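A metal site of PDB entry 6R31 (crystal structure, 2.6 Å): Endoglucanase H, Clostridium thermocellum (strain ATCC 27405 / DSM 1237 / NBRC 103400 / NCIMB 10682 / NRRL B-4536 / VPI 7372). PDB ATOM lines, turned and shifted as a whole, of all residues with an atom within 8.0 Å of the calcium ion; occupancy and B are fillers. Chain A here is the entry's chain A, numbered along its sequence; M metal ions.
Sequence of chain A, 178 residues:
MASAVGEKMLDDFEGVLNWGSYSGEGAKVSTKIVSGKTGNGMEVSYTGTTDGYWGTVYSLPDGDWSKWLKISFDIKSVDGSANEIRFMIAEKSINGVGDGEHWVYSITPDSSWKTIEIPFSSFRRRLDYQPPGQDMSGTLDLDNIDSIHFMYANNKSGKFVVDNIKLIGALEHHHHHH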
ATOM      1  N   GLU A  91      16.837 -11.359 -24.334  1.00  0.00           N
ATOM      2  CA  GLU A  91      17.967 -11.052 -25.208  1.00  0.00           C
ATOM      3  C   GLU A  91      19.074 -10.371 -24.405  1.00  0.00           C
ATOM      4  O   GLU A  91      18.904 -10.080 -23.217  1.00  0.00           O
ATOM      5  CB  GLU A  91      17.535 -10.146 -26.362  1.00  0.00           C
ATOM      6  CG  GLU A  91      16.332 -10.688 -27.119  1.00  0.00           C
ATOM      7  CD  GLU A  91      15.885  -9.828 -28.280  1.00  0.00           C
ATOM      8  OE1 GLU A  91      16.281  -8.654 -28.351  1.00  0.00           O
ATOM      9  OE2 GLU A  91      15.128 -10.339 -29.116  1.00  0.00           O
ATOM     10  N   LYS A  92      20.220 -10.109 -25.036  1.00  0.00           N
ATOM     11  CA  LYS A  92      21.320  -9.479 -24.317  1.00  0.00           C
ATOM     12  C   LYS A  92      21.086  -7.965 -24.257  1.00  0.00           C
ATOM     13  O   LYS A  92      20.371  -7.409 -25.090  1.00  0.00           O
ATOM     14  CB  LYS A  92      22.679  -9.852 -24.912  1.00  0.00           C
ATOM     15  CG  LYS A  92      23.053 -11.293 -24.668  1.00  0.00           C
ATOM     16  CD  LYS A  92      24.138 -11.858 -25.539  1.00  0.00           C
ATOM     17  CE  LYS A  92      24.720 -13.081 -24.849  1.00  0.00           C
ATOM     18  NZ  LYS A  92      25.838 -13.702 -25.584  1.00  0.00           N
ATOM     19  N   ILE A  94      21.673  -3.926 -24.526  1.00  0.00           N
ATOM     20  CA  ILE A  94      22.280  -3.050 -25.515  1.00  0.00           C
ATOM     21  C   ILE A  94      23.196  -2.037 -24.831  1.00  0.00           C
ATOM     22  O   ILE A  94      23.846  -1.257 -25.507  1.00  0.00           O
ATOM     23  CB  ILE A  94      21.210  -2.378 -26.402  1.00  0.00           C
ATOM     24  CG1 ILE A  94      20.278  -1.472 -25.602  1.00  0.00           C
ATOM     25  CG2 ILE A  94      20.424  -3.403 -27.216  1.00  0.00           C
ATOM     26  CD1 ILE A  94      20.636  -0.008 -25.685  1.00  0.00           C
ATOM     27  N   GLY A 100      18.056  -7.870 -21.694  1.00  0.00           N
ATOM     28  CA  GLY A 100      17.357  -7.169 -22.745  1.00  0.00           C
ATOM     29  C   GLY A 100      15.912  -7.623 -22.888  1.00  0.00           C
ATOM     30  O   GLY A 100      15.299  -8.043 -21.902  1.00  0.00           O
ATOM     31  N   GLU A 101      15.402  -7.533 -24.126  1.00  0.00           N
ATOM     32  CA  GLU A 101      13.990  -7.638 -24.455  1.00  0.00           C
ATOM     33  C   GLU A 101      13.439  -8.994 -24.028  1.00  0.00           C
ATOM     34  O   GLU A 101      14.018 -10.029 -24.354  1.00  0.00           O
ATOM     35  CB  GLU A 101      13.811  -7.376 -25.955  1.00  0.00           C
ATOM     36  CG  GLU A 101      12.401  -6.980 -26.360  1.00  0.00           C
ATOM     37  CD  GLU A 101      12.184  -6.826 -27.865  1.00  0.00           C
ATOM     38  OE1 GLU A 101      12.918  -7.478 -28.648  1.00  0.00           O
ATOM     39  OE2 GLU A 101      11.293  -6.056 -28.242  1.00  0.00           O
ATOM     40  N   HIS A 102      12.312  -8.962 -23.300  1.00  0.00           N
ATOM     41  CA  HIS A 102      11.740 -10.152 -22.658  1.00  0.00           C
ATOM     42  C   HIS A 102      10.639 -10.760 -23.523  1.00  0.00           C
ATOM     43  O   HIS A 102       9.730 -10.048 -23.956  1.00  0.00           O
ATOM     44  CB  HIS A 102      11.122  -9.797 -21.304  1.00  0.00           C
ATOM     45  CG  HIS A 102      12.107  -9.539 -20.211  1.00  0.00           C
ATOM     46  ND1 HIS A 102      11.781  -8.803 -19.091  1.00  0.00           N
ATOM     47  CD2 HIS A 102      13.391  -9.919 -20.061  1.00  0.00           C
ATOM     48  CE1 HIS A 102      12.827  -8.737 -18.291  1.00  0.00           C
ATOM     49  NE2 HIS A 102      13.820  -9.422 -18.852  1.00  0.00           N
ATOM     50  N   TRP A 103      10.696 -12.082 -23.705  1.00  0.00           N
ATOM     51  CA  TRP A 103       9.785 -12.806 -24.566  1.00  0.00           C
ATOM     52  C   TRP A 103       9.145 -13.967 -23.804  1.00  0.00           C
ATOM     53  O   TRP A 103       9.840 -14.802 -23.226  1.00  0.00           O
ATOM     54  CB  TRP A 103      10.500 -13.249 -25.849  1.00  0.00           C
ATOM     55  CG  TRP A 103      10.797 -12.100 -26.754  1.00  0.00           C
ATOM     56  CD1 TRP A 103      11.854 -11.242 -26.685  1.00  0.00           C
ATOM     57  CD2 TRP A 103       9.980 -11.640 -27.852  1.00  0.00           C
ATOM     58  NE1 TRP A 103      11.769 -10.296 -27.671  1.00  0.00           N
ATOM     59  CE2 TRP A 103      10.631 -10.514 -28.400  1.00  0.00           C
ATOM     60  CE3 TRP A 103       8.774 -12.077 -28.415  1.00  0.00           C
ATOM     61  CZ2 TRP A 103      10.105  -9.823 -29.491  1.00  0.00           C
ATOM     62  CZ3 TRP A 103       8.255 -11.388 -29.490  1.00  0.00           C
ATOM     63  CH2 TRP A 103       8.921 -10.272 -30.026  1.00  0.00           C
ATOM     64  N   ARG A 125       6.058 -10.808 -27.026  1.00  0.00           N
ATOM     65  CA  ARG A 125       6.807  -9.809 -26.282  1.00  0.00           C
ATOM     66  C   ARG A 125       6.083  -9.539 -24.967  1.00  0.00           C
ATOM     67  O   ARG A 125       4.870  -9.425 -24.953  1.00  0.00           O
ATOM     68  CB  ARG A 125       6.923  -8.541 -27.136  1.00  0.00           C
ATOM     69  CG  ARG A 125       7.880  -7.508 -26.569  1.00  0.00           C
ATOM     70  CD  ARG A 125       7.740  -6.189 -27.298  1.00  0.00           C
ATOM     71  NE  ARG A 125       6.449  -5.568 -27.026  1.00  0.00           N
ATOM     72  CZ  ARG A 125       6.199  -4.755 -26.018  1.00  0.00           C
ATOM     73  NH1 ARG A 125       7.146  -4.457 -25.147  1.00  0.00           N
ATOM     74  NH2 ARG A 125       4.993  -4.231 -25.876  1.00  0.00           N
ATOM     75  N   GLN A 134      16.775  -3.076 -23.134  1.00  0.00           N
ATOM     76  CA  GLN A 134      16.144  -3.776 -24.257  1.00  0.00           C
ATOM     77  C   GLN A 134      16.384  -3.078 -25.597  1.00  0.00           C
ATOM     78  O   GLN A 134      16.535  -1.865 -25.641  1.00  0.00           O
ATOM     79  CB  GLN A 134      14.642  -3.973 -23.988  1.00  0.00           C
ATOM     80  CG  GLN A 134      13.835  -2.687 -23.894  1.00  0.00           C
ATOM     81  CD  GLN A 134      12.532  -2.778 -24.633  1.00  0.00           C
ATOM     82  OE1 GLN A 134      12.360  -3.601 -25.537  1.00  0.00           O
ATOM     83  NE2 GLN A 134      11.591  -1.920 -24.269  1.00  0.00           N
ATOM     84  N   ASP A 135      16.386  -3.853 -26.690  1.00  0.00           N
ATOM     85  CA  ASP A 135      16.634  -3.301 -28.014  1.00  0.00           C
ATOM     86  C   ASP A 135      15.368  -2.624 -28.537  1.00  0.00           C
ATOM     87  O   ASP A 135      15.456  -1.747 -29.391  1.00  0.00           O
ATOM     88  CB  ASP A 135      17.176  -4.339 -29.002  1.00  0.00           C
ATOM     89  CG  ASP A 135      16.162  -5.380 -29.462  1.00  0.00           C
ATOM     90  OD1 ASP A 135      14.956  -5.199 -29.244  1.00  0.00           O
ATOM     91  OD2 ASP A 135      16.598  -6.387 -30.055  1.00  0.00           O
ATOM     92  N   MET A 136      14.201  -3.070 -28.050  1.00  0.00           N
ATOM     93  CA  MET A 136      12.930  -2.499 -28.448  1.00  0.00           C
ATOM     94  C   MET A 136      12.688  -2.744 -29.949  1.00  0.00           C
ATOM     95  O   MET A 136      12.120  -1.906 -30.647  1.00  0.00           O
ATOM     96  CB  MET A 136      12.907  -0.996 -28.114  1.00  0.00           C
ATOM     97  CG  MET A 136      11.670  -0.534 -27.349  1.00  0.00           C
ATOM     98  SD  MET A 136      11.719   1.176 -26.682  1.00  0.00           S
ATOM     99  CE  MET A 136      13.125   1.076 -25.558  1.00  0.00           C
ATOM    100  N   SER A 137      13.089  -3.915 -30.456  1.00  0.00           N
ATOM    101  CA  SER A 137      13.032  -4.222 -31.878  1.00  0.00           C
ATOM    102  C   SER A 137      11.657  -4.763 -32.281  1.00  0.00           C
ATOM    103  O   SER A 137      11.301  -4.736 -33.459  1.00  0.00           O
ATOM    104  CB  SER A 137      14.137  -5.167 -32.307  1.00  0.00           C
ATOM    105  OG  SER A 137      13.945  -6.475 -31.789  1.00  0.00           O
ATOM    106  N   GLY A 138      10.920  -5.303 -31.307  1.00  0.00           N
ATOM    107  CA  GLY A 138       9.653  -5.973 -31.579  1.00  0.00           C
ATOM    108  C   GLY A 138       9.857  -7.351 -32.213  1.00  0.00           C
ATOM    109  O   GLY A 138       8.897  -8.002 -32.620  1.00  0.00           O
ATOM    110  N   THR A 139      11.125  -7.783 -32.273  1.00  0.00           N
ATOM    111  CA  THR A 139      11.522  -9.051 -32.859  1.00  0.00           C
ATOM    112  C   THR A 139      12.304  -9.840 -31.806  1.00  0.00           C
ATOM    113  O   THR A 139      12.931  -9.249 -30.931  1.00  0.00           O
ATOM    114  CB  THR A 139      12.350  -8.852 -34.142  1.00  0.00           C
ATOM    115  OG1 THR A 139      13.583  -8.207 -33.830  1.00  0.00           O
ATOM    116  CG2 THR A 139      11.593  -8.081 -35.213  1.00  0.00           C
ATOM    117  N   LEU A 140      12.228 -11.163 -31.884  1.00  0.00           N
ATOM    118  CA  LEU A 140      13.060 -12.023 -31.056  1.00  0.00           C
ATOM    119  C   LEU A 140      14.318 -12.374 -31.841  1.00  0.00           C
ATOM    120  O   LEU A 140      14.236 -13.049 -32.877  1.00  0.00           O
ATOM    121  CB  LEU A 140      12.250 -13.256 -30.642  1.00  0.00           C
ATOM    122  CG  LEU A 140      13.020 -14.285 -29.819  1.00  0.00           C
ATOM    123  CD1 LEU A 140      13.846 -13.606 -28.734  1.00  0.00           C
ATOM    124  CD2 LEU A 140      12.071 -15.319 -29.224  1.00  0.00           C
ATOM    125  N   ASP A 141      15.477 -11.896 -31.348  1.00  0.00           N
ATOM    126  CA  ASP A 141      16.755 -12.003 -32.042  1.00  0.00           C
ATOM    127  C   ASP A 141      17.558 -13.189 -31.509  1.00  0.00           C
ATOM    128  O   ASP A 141      18.272 -13.074 -30.526  1.00  0.00           O
ATOM    129  CB  ASP A 141      17.548 -10.692 -31.920  1.00  0.00           C
ATOM    130  CG  ASP A 141      16.721  -9.473 -32.290  1.00  0.00           C
ATOM    131  OD1 ASP A 141      16.468  -9.306 -33.496  1.00  0.00           O
ATOM    132  OD2 ASP A 141      16.353  -8.712 -31.369  1.00  0.00           O
ATOM    133  N   LEU A 142      17.472 -14.319 -32.223  1.00  0.00           N
ATOM    134  CA  LEU A 142      17.965 -15.607 -31.768  1.00  0.00           C
ATOM    135  C   LEU A 142      19.487 -15.746 -31.887  1.00  0.00           C
ATOM    136  O   LEU A 142      20.027 -16.779 -31.518  1.00  0.00           O
ATOM    137  CB  LEU A 142      17.262 -16.721 -32.556  1.00  0.00           C
ATOM    138  CG  LEU A 142      15.769 -16.904 -32.295  1.00  0.00           C
ATOM    139  CD1 LEU A 142      15.032 -17.376 -33.543  1.00  0.00           C
ATOM    140  CD2 LEU A 142      15.526 -17.867 -31.140  1.00  0.00           C
ATOM    141  N   ASN A 144      21.194 -13.582 -30.189  1.00  0.00           N
ATOM    142  CA  ASN A 144      21.534 -12.649 -29.123  1.00  0.00           C
ATOM    143  C   ASN A 144      20.733 -12.924 -27.852  1.00  0.00           C
ATOM    144  O   ASN A 144      20.176 -11.994 -27.262  1.00  0.00           O
ATOM    145  CB  ASN A 144      21.314 -11.199 -29.565  1.00  0.00           C
ATOM    146  CG  ASN A 144      22.183 -10.224 -28.800  1.00  0.00           C
ATOM    147  OD1 ASN A 144      23.386 -10.444 -28.656  1.00  0.00           O
ATOM    148  ND2 ASN A 144      21.588  -9.143 -28.319  1.00  0.00           N
HETATM  149 CA    CA M   1      14.629  -7.769 -30.075  1.00  0.00          CA
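The calcium ion is bound by OE1 of Glu 101 (2.2 Å), OG of Ser 137 (2.3 Å), OD2 of Asp 141 (2.4 Å), OD2 of Asp 135 (2.4 Å), O of Thr 139 (2.4 Å), OE1 of Glu 91 (2.5 Å), OD1 of Asp 135 (2.7 Å) and OE2 of Glu 91 (2.8 Å). The calcium ion has eight donor atoms within binding distance.
Within 4 Å of the calcium ion: Glu 91, Glu 101, Asp 135, Ser 137, Thr 139 and Asp 141. The nearest printed residue that does not touch the calcium ion is Trp 103 (4.5 Å).
O of Glu 91 lies within hydrogen-bond range of N of Gly 100 (2.8 Å). OE2 of Glu 101 sits at hydrogen-bond distance from N of Gly 138 (3.2 Å). The side-chain carboxylate (OE1) of Glu 101 lies close to the indole nitrogen (NE1) of Trp 103 (3.2 Å).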
